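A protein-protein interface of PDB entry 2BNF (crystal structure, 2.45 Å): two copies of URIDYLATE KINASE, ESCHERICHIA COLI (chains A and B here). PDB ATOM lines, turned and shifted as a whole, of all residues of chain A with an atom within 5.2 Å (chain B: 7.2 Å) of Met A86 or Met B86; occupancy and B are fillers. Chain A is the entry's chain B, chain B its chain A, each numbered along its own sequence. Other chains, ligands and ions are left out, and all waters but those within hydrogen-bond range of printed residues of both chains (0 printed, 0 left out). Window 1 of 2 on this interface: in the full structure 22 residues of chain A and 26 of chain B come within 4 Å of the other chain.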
ATOM      1  N   ILE A  29      13.590  -7.503  16.966  1.00  0.00           N
ATOM      2  CA  ILE A  29      12.560  -8.213  17.726  1.00  0.00           C
ATOM      3  C   ILE A  29      12.557  -7.828  19.200  1.00  0.00           C
ATOM      4  O   ILE A  29      13.590  -7.495  19.768  1.00  0.00           O
ATOM      5  CB  ILE A  29      12.752  -9.749  17.642  1.00  0.00           C
ATOM      6  CG1 ILE A  29      12.626 -10.218  16.192  1.00  0.00           C
ATOM      7  CG2 ILE A  29      11.718 -10.456  18.505  1.00  0.00           C
ATOM      8  CD1 ILE A  29      12.800 -11.708  16.032  1.00  0.00           C
ATOM      9  N   LEU A  60      11.775  -5.962   9.522  1.00  0.00           N
ATOM     10  CA  LEU A  60      13.125  -6.138   8.989  1.00  0.00           C
ATOM     11  C   LEU A  60      13.232  -5.623   7.548  1.00  0.00           C
ATOM     12  O   LEU A  60      14.043  -4.743   7.269  1.00  0.00           O
ATOM     13  CB  LEU A  60      13.531  -7.615   9.055  1.00  0.00           C
ATOM     14  CG  LEU A  60      13.482  -8.256  10.450  1.00  0.00           C
ATOM     15  CD1 LEU A  60      13.850  -9.733  10.365  1.00  0.00           C
ATOM     16  CD2 LEU A  60      14.427  -7.517  11.383  1.00  0.00           C
ATOM     17  N   PHE A  61      12.410  -6.155   6.643  1.00  0.00           N
ATOM     18  CA  PHE A  61      12.429  -5.734   5.240  1.00  0.00           C
ATOM     19  C   PHE A  61      11.090  -5.842   4.507  1.00  0.00           C
ATOM     20  O   PHE A  61      10.285  -6.736   4.768  1.00  0.00           O
ATOM     21  CB  PHE A  61      13.467  -6.542   4.444  1.00  0.00           C
ATOM     22  CG  PHE A  61      14.881  -6.286   4.857  1.00  0.00           C
ATOM     23  CD1 PHE A  61      15.641  -7.293   5.456  1.00  0.00           C
ATOM     24  CD2 PHE A  61      15.448  -5.024   4.686  1.00  0.00           C
ATOM     25  CE1 PHE A  61      16.945  -7.042   5.885  1.00  0.00           C
ATOM     26  CE2 PHE A  61      16.749  -4.758   5.111  1.00  0.00           C
ATOM     27  CZ  PHE A  61      17.502  -5.765   5.712  1.00  0.00           C
ATOM     28  N   MET A  79      13.930 -11.091   0.220  1.00  0.00           N
ATOM     29  CA  MET A  79      14.521 -10.742   1.500  1.00  0.00           C
ATOM     30  C   MET A  79      13.395 -10.543   2.493  1.00  0.00           C
ATOM     31  O   MET A  79      13.501 -10.913   3.659  1.00  0.00           O
ATOM     32  CB  MET A  79      15.361  -9.475   1.370  1.00  0.00           C
ATOM     33  CG  MET A  79      16.765  -9.756   0.858  1.00  0.00           C
ATOM     34  SD  MET A  79      17.649  -8.214   0.158  1.00  0.00           S
ATOM     35  CE  MET A  79      18.007  -7.335   1.859  1.00  0.00           C
ATOM     36  N   LEU A  82      12.510 -13.896   3.666  1.00  0.00           N
ATOM     37  CA  LEU A  82      13.473 -14.450   4.615  1.00  0.00           C
ATOM     38  C   LEU A  82      13.288 -13.774   5.971  1.00  0.00           C
ATOM     39  O   LEU A  82      13.596 -14.357   7.016  1.00  0.00           O
ATOM     40  CB  LEU A  82      14.910 -14.239   4.131  1.00  0.00           C
ATOM     41  CG  LEU A  82      15.287 -15.155   2.965  1.00  0.00           C
ATOM     42  CD1 LEU A  82      16.605 -14.716   2.338  1.00  0.00           C
ATOM     43  CD2 LEU A  82      15.371 -16.586   3.469  1.00  0.00           C
ATOM     44  N   ALA A  83      12.778 -12.545   5.947  1.00  0.00           N
ATOM     45  CA  ALA A  83      12.538 -11.800   7.169  1.00  0.00           C
ATOM     46  C   ALA A  83      11.403 -12.485   7.933  1.00  0.00           C
ATOM     47  O   ALA A  83      11.444 -12.578   9.156  1.00  0.00           O
ATOM     48  CB  ALA A  83      12.177 -10.355   6.842  1.00  0.00           C
ATOM     49  N   THR A  84      10.400 -12.986   7.213  1.00  0.00           N
ATOM     50  CA  THR A  84       9.297 -13.658   7.883  1.00  0.00           C
ATOM     51  C   THR A  84       9.780 -14.992   8.459  1.00  0.00           C
ATOM     52  O   THR A  84       9.274 -15.464   9.480  1.00  0.00           O
ATOM     53  CB  THR A  84       8.103 -13.900   6.940  1.00  0.00           C
ATOM     54  OG1 THR A  84       8.436 -14.907   5.967  1.00  0.00           O
ATOM     55  CG2 THR A  84       7.718 -12.599   6.240  1.00  0.00           C
ATOM     56  N   VAL A  85      10.772 -15.595   7.819  1.00  0.00           N
ATOM     57  CA  VAL A  85      11.300 -16.854   8.318  1.00  0.00           C
ATOM     58  C   VAL A  85      12.106 -16.602   9.589  1.00  0.00           C
ATOM     59  O   VAL A  85      12.153 -17.449  10.467  1.00  0.00           O
ATOM     60  CB  VAL A  85      12.168 -17.573   7.242  1.00  0.00           C
ATOM     61  CG1 VAL A  85      12.836 -18.809   7.820  1.00  0.00           C
ATOM     62  CG2 VAL A  85      11.282 -17.962   6.061  1.00  0.00           C
ATOM     63  N   MET A  86      12.720 -15.432   9.708  1.00  0.00           N
ATOM     64  CA  MET A  86      13.492 -15.136  10.915  1.00  0.00           C
ATOM     65  C   MET A  86      12.555 -14.913  12.095  1.00  0.00           C
ATOM     66  O   MET A  86      12.860 -15.301  13.221  1.00  0.00           O
ATOM     67  CB  MET A  86      14.385 -13.910  10.709  1.00  0.00           C
ATOM     68  CG  MET A  86      15.828 -14.266  10.376  1.00  0.00           C
ATOM     69  SD  MET A  86      16.677 -13.077   9.077  1.00  0.00           S
ATOM     70  CE  MET A  86      17.585 -11.892  10.303  1.00  0.00           C
ATOM     71  N   ASN A  87      11.408 -14.291  11.829  1.00  0.00           N
ATOM     72  CA  ASN A  87      10.422 -14.036  12.871  1.00  0.00           C
ATOM     73  C   ASN A  87       9.783 -15.360  13.261  1.00  0.00           C
ATOM     74  O   ASN A  87       9.618 -15.647  14.435  1.00  0.00           O
ATOM     75  CB  ASN A  87       9.337 -13.062  12.386  1.00  0.00           C
ATOM     76  CG  ASN A  87       9.858 -11.642  12.190  1.00  0.00           C
ATOM     77  OD1 ASN A  87      10.712 -11.172  12.939  1.00  0.00           O
ATOM     78  ND2 ASN A  87       9.325 -10.948  11.196  1.00  0.00           N
ATOM     79  N   GLY A  88       9.449 -16.170  12.262  1.00  0.00           N
ATOM     80  CA  GLY A  88       8.836 -17.460  12.521  1.00  0.00           C
ATOM     81  C   GLY A  88       9.708 -18.323  13.413  1.00  0.00           C
ATOM     82  O   GLY A  88       9.213 -19.022  14.293  1.00  0.00           O
ATOM     83  N   LEU A  89      11.015 -18.269  13.180  1.00  0.00           N
ATOM     84  CA  LEU A  89      11.995 -19.039  13.953  1.00  0.00           C
ATOM     85  C   LEU A  89      12.053 -18.530  15.400  1.00  0.00           C
ATOM     86  O   LEU A  89      12.122 -19.318  16.337  1.00  0.00           O
ATOM     87  CB  LEU A  89      13.361 -18.907  13.284  1.00  0.00           C
ATOM     88  CG  LEU A  89      14.527 -19.828  13.613  1.00  0.00           C
ATOM     89  CD1 LEU A  89      14.110 -21.292  13.528  1.00  0.00           C
ATOM     90  CD2 LEU A  89      15.641 -19.539  12.609  1.00  0.00           C
ATOM     91  N   ALA A  90      12.027 -17.211  15.580  1.00  0.00           N
ATOM     92  CA  ALA A  90      12.049 -16.640  16.916  1.00  0.00           C
ATOM     93  C   ALA A  90      10.738 -17.001  17.619  1.00  0.00           C
ATOM     94  O   ALA A  90      10.741 -17.386  18.778  1.00  0.00           O
ATOM     95  CB  ALA A  90      12.210 -15.134  16.839  1.00  0.00           C
ATOM     96  N   MET A  91       9.617 -16.889  16.906  1.00  0.00           N
ATOM     97  CA  MET A  91       8.318 -17.209  17.483  1.00  0.00           C
ATOM     98  C   MET A  91       8.285 -18.670  17.937  1.00  0.00           C
ATOM     99  O   MET A  91       7.920 -18.959  19.067  1.00  0.00           O
ATOM    100  CB  MET A  91       7.200 -16.930  16.468  1.00  0.00           C
ATOM    101  CG  MET A  91       5.772 -17.216  16.969  1.00  0.00           C
ATOM    102  SD  MET A  91       5.206 -16.231  18.563  1.00  0.00           S
ATOM    103  CE  MET A  91       5.237 -14.458  17.825  1.00  0.00           C
ATOM    104  N   LEU B  21      27.697  -3.071   5.681  1.00  0.00           N
ATOM    105  CA  LEU B  21      26.572  -2.621   4.866  1.00  0.00           C
ATOM    106  C   LEU B  21      25.648  -1.662   5.626  1.00  0.00           C
ATOM    107  O   LEU B  21      24.691  -1.135   5.058  1.00  0.00           O
ATOM    108  CB  LEU B  21      25.753  -3.825   4.382  1.00  0.00           C
ATOM    109  CG  LEU B  21      26.469  -5.115   3.967  1.00  0.00           C
ATOM    110  CD1 LEU B  21      25.468  -6.006   3.255  1.00  0.00           C
ATOM    111  CD2 LEU B  21      27.644  -4.826   3.056  1.00  0.00           C
ATOM    112  N   ILE B  29      20.665  -2.431   5.859  1.00  0.00           N
ATOM    113  CA  ILE B  29      21.487  -2.246   4.675  1.00  0.00           C
ATOM    114  C   ILE B  29      21.309  -0.852   4.078  1.00  0.00           C
ATOM    115  O   ILE B  29      20.209  -0.316   4.052  1.00  0.00           O
ATOM    116  CB  ILE B  29      21.109  -3.301   3.624  1.00  0.00           C
ATOM    117  CG1 ILE B  29      21.254  -4.692   4.239  1.00  0.00           C
ATOM    118  CG2 ILE B  29      21.979  -3.160   2.384  1.00  0.00           C
ATOM    119  CD1 ILE B  29      20.607  -5.788   3.439  1.00  0.00           C
ATOM    120  N   ILE B  55      30.207 -12.810   3.957  1.00  0.00           N
ATOM    121  CA  ILE B  55      29.633 -11.682   4.661  1.00  0.00           C
ATOM    122  C   ILE B  55      28.980 -12.066   5.994  1.00  0.00           C
ATOM    123  O   ILE B  55      28.401 -13.145   6.123  1.00  0.00           O
ATOM    124  CB  ILE B  55      28.628 -10.940   3.745  1.00  0.00           C
ATOM    125  CG1 ILE B  55      27.902  -9.862   4.541  1.00  0.00           C
ATOM    126  CG2 ILE B  55      27.646 -11.925   3.133  1.00  0.00           C
ATOM    127  CD1 ILE B  55      27.427  -8.693   3.702  1.00  0.00           C
ATOM    128  N   GLY B  56      29.090 -11.172   6.980  1.00  0.00           N
ATOM    129  CA  GLY B  56      28.527 -11.428   8.299  1.00  0.00           C
ATOM    130  C   GLY B  56      27.095 -10.960   8.463  1.00  0.00           C
ATOM    131  O   GLY B  56      26.459 -10.569   7.491  1.00  0.00           O
ATOM    132  N   GLY B  57      26.585 -10.998   9.693  1.00  0.00           N
ATOM    133  CA  GLY B  57      25.212 -10.581   9.935  1.00  0.00           C
ATOM    134  C   GLY B  57      24.996  -9.664  11.132  1.00  0.00           C
ATOM    135  O   GLY B  57      23.867  -9.482  11.581  1.00  0.00           O
ATOM    136  N   LEU B  60      22.227  -7.138  11.786  1.00  0.00           N
ATOM    137  CA  LEU B  60      20.900  -7.694  11.986  1.00  0.00           C
ATOM    138  C   LEU B  60      20.803  -8.547  13.258  1.00  0.00           C
ATOM    139  O   LEU B  60      20.048  -8.209  14.163  1.00  0.00           O
ATOM    140  CB  LEU B  60      20.494  -8.514  10.760  1.00  0.00           C
ATOM    141  CG  LEU B  60      20.386  -7.748   9.437  1.00  0.00           C
ATOM    142  CD1 LEU B  60      20.261  -8.720   8.272  1.00  0.00           C
ATOM    143  CD2 LEU B  60      19.195  -6.820   9.488  1.00  0.00           C
ATOM    144  N   PHE B  61      21.568  -9.634  13.342  1.00  0.00           N
ATOM    145  CA  PHE B  61      21.502 -10.501  14.520  1.00  0.00           C
ATOM    146  C   PHE B  61      22.795 -11.195  14.930  1.00  0.00           C
ATOM    147  O   PHE B  61      23.676 -11.446  14.111  1.00  0.00           O
ATOM    148  CB  PHE B  61      20.433 -11.579  14.323  1.00  0.00           C
ATOM    149  CG  PHE B  61      19.029 -11.070  14.424  1.00  0.00           C
ATOM    150  CD1 PHE B  61      18.132 -11.261  13.380  1.00  0.00           C
ATOM    151  CD2 PHE B  61      18.594 -10.407  15.568  1.00  0.00           C
ATOM    152  CE1 PHE B  61      16.820 -10.799  13.470  1.00  0.00           C
ATOM    153  CE2 PHE B  61      17.287  -9.940  15.670  1.00  0.00           C
ATOM    154  CZ  PHE B  61      16.398 -10.135  14.621  1.00  0.00           C
ATOM    155  N   MET B  71      16.551 -16.504  24.546  1.00  0.00           N
ATOM    156  CA  MET B  71      16.455 -17.453  23.437  1.00  0.00           C
ATOM    157  C   MET B  71      17.472 -18.597  23.426  1.00  0.00           C
ATOM    158  O   MET B  71      18.560 -18.479  23.985  1.00  0.00           O
ATOM    159  CB  MET B  71      16.553 -16.675  22.130  1.00  0.00           C
ATOM    160  CG  MET B  71      16.293 -17.478  20.886  1.00  0.00           C
ATOM    161  SD  MET B  71      16.042 -16.270  19.416  1.00  0.00           S
ATOM    162  CE  MET B  71      14.318 -15.569  19.931  1.00  0.00           C
ATOM    163  N   VAL B  75      19.249 -21.571  18.195  1.00  0.00           N
ATOM    164  CA  VAL B  75      18.267 -20.908  17.353  1.00  0.00           C
ATOM    165  C   VAL B  75      18.733 -19.484  17.048  1.00  0.00           C
ATOM    166  O   VAL B  75      18.477 -18.957  15.967  1.00  0.00           O
ATOM    167  CB  VAL B  75      16.890 -20.869  18.036  1.00  0.00           C
ATOM    168  CG1 VAL B  75      15.934 -20.009  17.227  1.00  0.00           C
ATOM    169  CG2 VAL B  75      16.345 -22.279  18.160  1.00  0.00           C
ATOM    170  N   HIS B  78      21.112 -19.624  14.323  1.00  0.00           N
ATOM    171  CA  HIS B  78      20.485 -19.922  13.035  1.00  0.00           C
ATOM    172  C   HIS B  78      19.960 -18.630  12.426  1.00  0.00           C
ATOM    173  O   HIS B  78      20.068 -18.406  11.217  1.00  0.00           O
ATOM    174  CB  HIS B  78      19.342 -20.925  13.200  1.00  0.00           C
ATOM    175  CG  HIS B  78      19.801 -22.345  13.305  1.00  0.00           C
ATOM    176  ND1 HIS B  78      18.973 -23.369  13.711  1.00  0.00           N
ATOM    177  CD2 HIS B  78      21.002 -22.916  13.045  1.00  0.00           C
ATOM    178  CE1 HIS B  78      19.643 -24.508  13.697  1.00  0.00           C
ATOM    179  NE2 HIS B  78      20.876 -24.260  13.296  1.00  0.00           N
ATOM    180  N   MET B  79      19.401 -17.776  13.276  1.00  0.00           N
ATOM    181  CA  MET B  79      18.877 -16.503  12.828  1.00  0.00           C
ATOM    182  C   MET B  79      20.042 -15.633  12.378  1.00  0.00           C
ATOM    183  O   MET B  79      19.939 -14.909  11.396  1.00  0.00           O
ATOM    184  CB  MET B  79      18.091 -15.837  13.959  1.00  0.00           C
ATOM    185  CG  MET B  79      16.696 -16.435  14.151  1.00  0.00           C
ATOM    186  SD  MET B  79      15.800 -15.827  15.752  1.00  0.00           S
ATOM    187  CE  MET B  79      15.231 -14.095  15.106  1.00  0.00           C
ATOM    188  N   GLY B  80      21.156 -15.718  13.099  1.00  0.00           N
ATOM    189  CA  GLY B  80      22.327 -14.948  12.726  1.00  0.00           C
ATOM    190  C   GLY B  80      22.752 -15.378  11.331  1.00  0.00           C
ATOM    191  O   GLY B  80      22.892 -14.550  10.426  1.00  0.00           O
ATOM    192  N   MET B  81      22.939 -16.681  11.151  1.00  0.00           N
ATOM    193  CA  MET B  81      23.337 -17.210   9.855  1.00  0.00           C
ATOM    194  C   MET B  81      22.374 -16.743   8.775  1.00  0.00           C
ATOM    195  O   MET B  81      22.784 -16.249   7.736  1.00  0.00           O
ATOM    196  CB  MET B  81      23.395 -18.750   9.888  1.00  0.00           C
ATOM    197  CG  MET B  81      24.591 -19.284  10.646  1.00  0.00           C
ATOM    198  SD  MET B  81      24.900 -21.188  10.513  1.00  0.00           S
ATOM    199  CE  MET B  81      24.007 -21.747  12.127  1.00  0.00           C
ATOM    200  N   LEU B  82      21.088 -16.881   9.043  1.00  0.00           N
ATOM    201  CA  LEU B  82      20.060 -16.486   8.091  1.00  0.00           C
ATOM    202  C   LEU B  82      20.159 -15.013   7.679  1.00  0.00           C
ATOM    203  O   LEU B  82      19.781 -14.642   6.565  1.00  0.00           O
ATOM    204  CB  LEU B  82      18.694 -16.782   8.695  1.00  0.00           C
ATOM    205  CG  LEU B  82      17.453 -16.739   7.820  1.00  0.00           C
ATOM    206  CD1 LEU B  82      17.682 -17.435   6.484  1.00  0.00           C
ATOM    207  CD2 LEU B  82      16.331 -17.420   8.607  1.00  0.00           C
ATOM    208  N   ALA B  83      20.680 -14.182   8.579  1.00  0.00           N
ATOM    209  CA  ALA B  83      20.846 -12.761   8.310  1.00  0.00           C
ATOM    210  C   ALA B  83      21.988 -12.563   7.314  1.00  0.00           C
ATOM    211  O   ALA B  83      21.945 -11.651   6.478  1.00  0.00           O
ATOM    212  CB  ALA B  83      21.147 -12.020   9.602  1.00  0.00           C
ATOM    213  N   THR B  84      23.004 -13.420   7.403  1.00  0.00           N
ATOM    214  CA  THR B  84      24.155 -13.328   6.503  1.00  0.00           C
ATOM    215  C   THR B  84      23.701 -13.696   5.098  1.00  0.00           C
ATOM    216  O   THR B  84      24.364 -13.379   4.110  1.00  0.00           O
ATOM    217  CB  THR B  84      25.297 -14.294   6.908  1.00  0.00           C
ATOM    218  OG1 THR B  84      24.943 -15.628   6.548  1.00  0.00           O
ATOM    219  CG2 THR B  84      25.549 -14.238   8.396  1.00  0.00           C
ATOM    220  N   VAL B  85      22.561 -14.371   5.011  1.00  0.00           N
ATOM    221  CA  VAL B  85      22.031 -14.754   3.715  1.00  0.00           C
ATOM    222  C   VAL B  85      21.233 -13.585   3.176  1.00  0.00           C
ATOM    223  O   VAL B  85      21.101 -13.422   1.966  1.00  0.00           O
ATOM    224  CB  VAL B  85      21.141 -16.005   3.810  1.00  0.00           C
ATOM    225  CG1 VAL B  85      20.546 -16.326   2.459  1.00  0.00           C
ATOM    226  CG2 VAL B  85      21.964 -17.183   4.308  1.00  0.00           C
ATOM    227  N   MET B  86      20.707 -12.764   4.076  1.00  0.00           N
ATOM    228  CA  MET B  86      19.941 -11.597   3.665  1.00  0.00           C
ATOM    229  C   MET B  86      20.933 -10.598   3.079  1.00  0.00           C
ATOM    230  O   MET B  86      20.653  -9.957   2.071  1.00  0.00           O
ATOM    231  CB  MET B  86      19.220 -10.994   4.863  1.00  0.00           C
ATOM    232  CG  MET B  86      17.731 -10.758   4.655  1.00  0.00           C
ATOM    233  SD  MET B  86      16.711 -11.195   6.267  1.00  0.00           S
ATOM    234  CE  MET B  86      17.395  -9.857   7.479  1.00  0.00           C
ATOM    235  N   ASN B  87      22.104 -10.493   3.710  1.00  0.00           N
ATOM    236  CA  ASN B  87      23.154  -9.594   3.248  1.00  0.00           C
ATOM    237  C   ASN B  87      23.745 -10.102   1.937  1.00  0.00           C
ATOM    238  O   ASN B  87      23.951  -9.331   1.000  1.00  0.00           O
ATOM    239  CB  ASN B  87      24.269  -9.465   4.303  1.00  0.00           C
ATOM    240  CG  ASN B  87      23.845  -8.632   5.518  1.00  0.00           C
ATOM    241  OD1 ASN B  87      23.094  -7.664   5.381  1.00  0.00           O
ATOM    242  ND2 ASN B  87      24.337  -8.997   6.699  1.00  0.00           N
ATOM    243  N   GLY B  88      24.007 -11.405   1.874  1.00  0.00           N
ATOM    244  CA  GLY B  88      24.576 -11.995   0.676  1.00  0.00           C
ATOM    245  C   GLY B  88      23.704 -11.814  -0.546  1.00  0.00           C
ATOM    246  O   GLY B  88      24.202 -11.686  -1.657  1.00  0.00           O
ATOM    247  N   LEU B  89      22.394 -11.795  -0.326  1.00  0.00           N
ATOM    248  CA  LEU B  89      21.391 -11.648  -1.378  1.00  0.00           C
ATOM    249  C   LEU B  89      21.356 -10.202  -1.897  1.00  0.00           C
ATOM    250  O   LEU B  89      21.215  -9.956  -3.097  1.00  0.00           O
ATOM    251  CB  LEU B  89      20.040 -12.038  -0.789  1.00  0.00           C
ATOM    252  CG  LEU B  89      18.913 -12.618  -1.631  1.00  0.00           C
ATOM    253  CD1 LEU B  89      19.434 -13.735  -2.505  1.00  0.00           C
ATOM    254  CD2 LEU B  89      17.822 -13.136  -0.687  1.00  0.00           C
ATOM    255  N   ALA B  90      21.480  -9.250  -0.980  1.00  0.00           N
ATOM    256  CA  ALA B  90      21.480  -7.836  -1.329  1.00  0.00           C
ATOM    257  C   ALA B  90      22.798  -7.490  -2.033  1.00  0.00           C
ATOM    258  O   ALA B  90      22.830  -6.685  -2.971  1.00  0.00           O
ATOM    259  CB  ALA B  90      21.316  -6.997  -0.073  1.00  0.00           C
ATOM    260  N   MET B  91      23.886  -8.095  -1.562  1.00  0.00           N
ATOM    261  CA  MET B  91      25.197  -7.869  -2.153  1.00  0.00           C
ATOM    262  C   MET B  91      25.225  -8.466  -3.559  1.00  0.00           C
ATOM    263  O   MET B  91      25.806  -7.890  -4.471  1.00  0.00           O
ATOM    264  CB  MET B  91      26.289  -8.499  -1.279  1.00  0.00           C
ATOM    265  CG  MET B  91      27.711  -8.467  -1.867  1.00  0.00           C
ATOM    266  SD  MET B  91      28.366  -6.700  -2.370  1.00  0.00           S
ATOM    267  CE  MET B  91      28.798  -6.045  -0.618  1.00  0.00           C
ATOM    268  N   ARG B  92      24.582  -9.612  -3.742  1.00  0.00           N
ATOM    269  CA  ARG B  92      24.569 -10.243  -5.051  1.00  0.00           C
ATOM    270  C   ARG B  92      23.795  -9.382  -6.027  1.00  0.00           C
ATOM    271  O   ARG B  92      24.198  -9.236  -7.177  1.00  0.00           O
ATOM    272  CB  ARG B  92      23.924 -11.624  -5.001  1.00  0.00           C
ATOM    273  CG  ARG B  92      24.005 -12.368  -6.329  1.00  0.00           C
ATOM    274  CD  ARG B  92      22.995 -13.498  -6.419  1.00  0.00           C
ATOM    275  NE  ARG B  92      21.617 -13.018  -6.509  1.00  0.00           N
ATOM    276  CZ  ARG B  92      20.546 -13.772  -6.289  1.00  0.00           C
ATOM    277  NH1 ARG B  92      20.687 -15.047  -5.954  1.00  0.00           N
ATOM    278  NH2 ARG B  92      19.331 -13.260  -6.423  1.00  0.00           N
ATOM    279  N   LEU B 104      25.242 -16.520  -5.329  1.00  0.00           N
ATOM    280  CA  LEU B 104      25.143 -16.643  -3.882  1.00  0.00           C
ATOM    281  C   LEU B 104      25.064 -18.118  -3.546  1.00  0.00           C
ATOM    282  O   LEU B 104      24.279 -18.848  -4.142  1.00  0.00           O
ATOM    283  CB  LEU B 104      23.882 -15.944  -3.365  1.00  0.00           C
ATOM    284  CG  LEU B 104      23.586 -15.976  -1.856  1.00  0.00           C
ATOM    285  CD1 LEU B 104      24.683 -15.266  -1.070  1.00  0.00           C
ATOM    286  CD2 LEU B 104      22.251 -15.298  -1.585  1.00  0.00           C
ATOM    287  N   SER B 135      27.316 -17.460   2.012  1.00  0.00           N
ATOM    288  CA  SER B 135      26.504 -17.115   3.164  1.00  0.00           C
ATOM    289  C   SER B 135      26.331 -18.260   4.162  1.00  0.00           C
ATOM    290  O   SER B 135      26.687 -19.407   3.882  1.00  0.00           O
ATOM    291  CB  SER B 135      25.128 -16.655   2.695  1.00  0.00           C
ATOM    292  OG  SER B 135      25.223 -15.429   2.001  1.00  0.00           O
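Met A86 touches just these residues of chain B: Phe B61, Met B79, Leu B82, Ala B83 and Met B86. Of the printed residues of chain A, Met B71 touches Ala A90 (3.8 Å). Printed residues of chain A within 4 Å of Leu B82: Leu A82 (3.9 Å), Val A85 (3.8 Å) and Met A86 (3.7 Å). Met B86 touches three residues of chain A. The nearest printed residue of chain A that does not touch Ala B90 is Phe A61 (7.0 Å).
The side-chain sulfur (SD) of Met A86 sits close to the side-chain sulfur (SD) of Met B86 (3.4 Å).
Of the 26 printed residues of chain B, 11 touch a printed residue of chain A. Hydrophobic or aromatic side chains of chain B that line the printed part of chain A: Ile B29, Phe B61, Met B71, Val B75, His B78, Met B79, Leu B82, Ala B83, Met B86, Leu B89 and Ala B90. Along chain B the printed residues that touch a printed residue of chain A span positions 29 to 90. Hydrophobic or aromatic side chains of chain A that line the printed part of chain B: Ile A29, Phe A61, Met A79, Leu A82, Val A85, Met A86, Leu A89 and Ala A90. Among the printed residues, 20 pairs touch across the chains. Among the printed residues, no Asp or Glu carboxylate lies within 4 Å of a Lys or Arg side-chain nitrogen of the other chain.
Ile A29 touches Met B79, and with the chains exchanged Met A79 touches Ile B29. Met A79 touches Met B86, and with the chains exchanged Met A86 touches Met B79. Met A79 touches Leu B89, and with the chains exchanged Leu A89 touches Met B79. Met A86 touches Leu B82, but with the chains exchanged Leu A82 does not touch Met B86 (4.1 Å). 14 positions are printed for both chains. Of the 20 pairs that touch across the chains among the printed residues, 12 have their exchanged pair printed and touching as well.
Met B86 touches Phe A61. Met A79 touches Ala B90. Val A85 touches Leu B82. CD1 of Phe B61 touches CE of Met A86, at 3.2 Å. Met A86 touches Met B79. Leu B82 touches Met A86. Ala B83 touches Met A86 (CB to CE, 3.6 Å). CB of His B78 touches CD2 of Leu A89, 3.996 Å away. Leu A89 touches Met B79. Ala A90 touches Met B71 (CB to CE, 3.8 Å).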
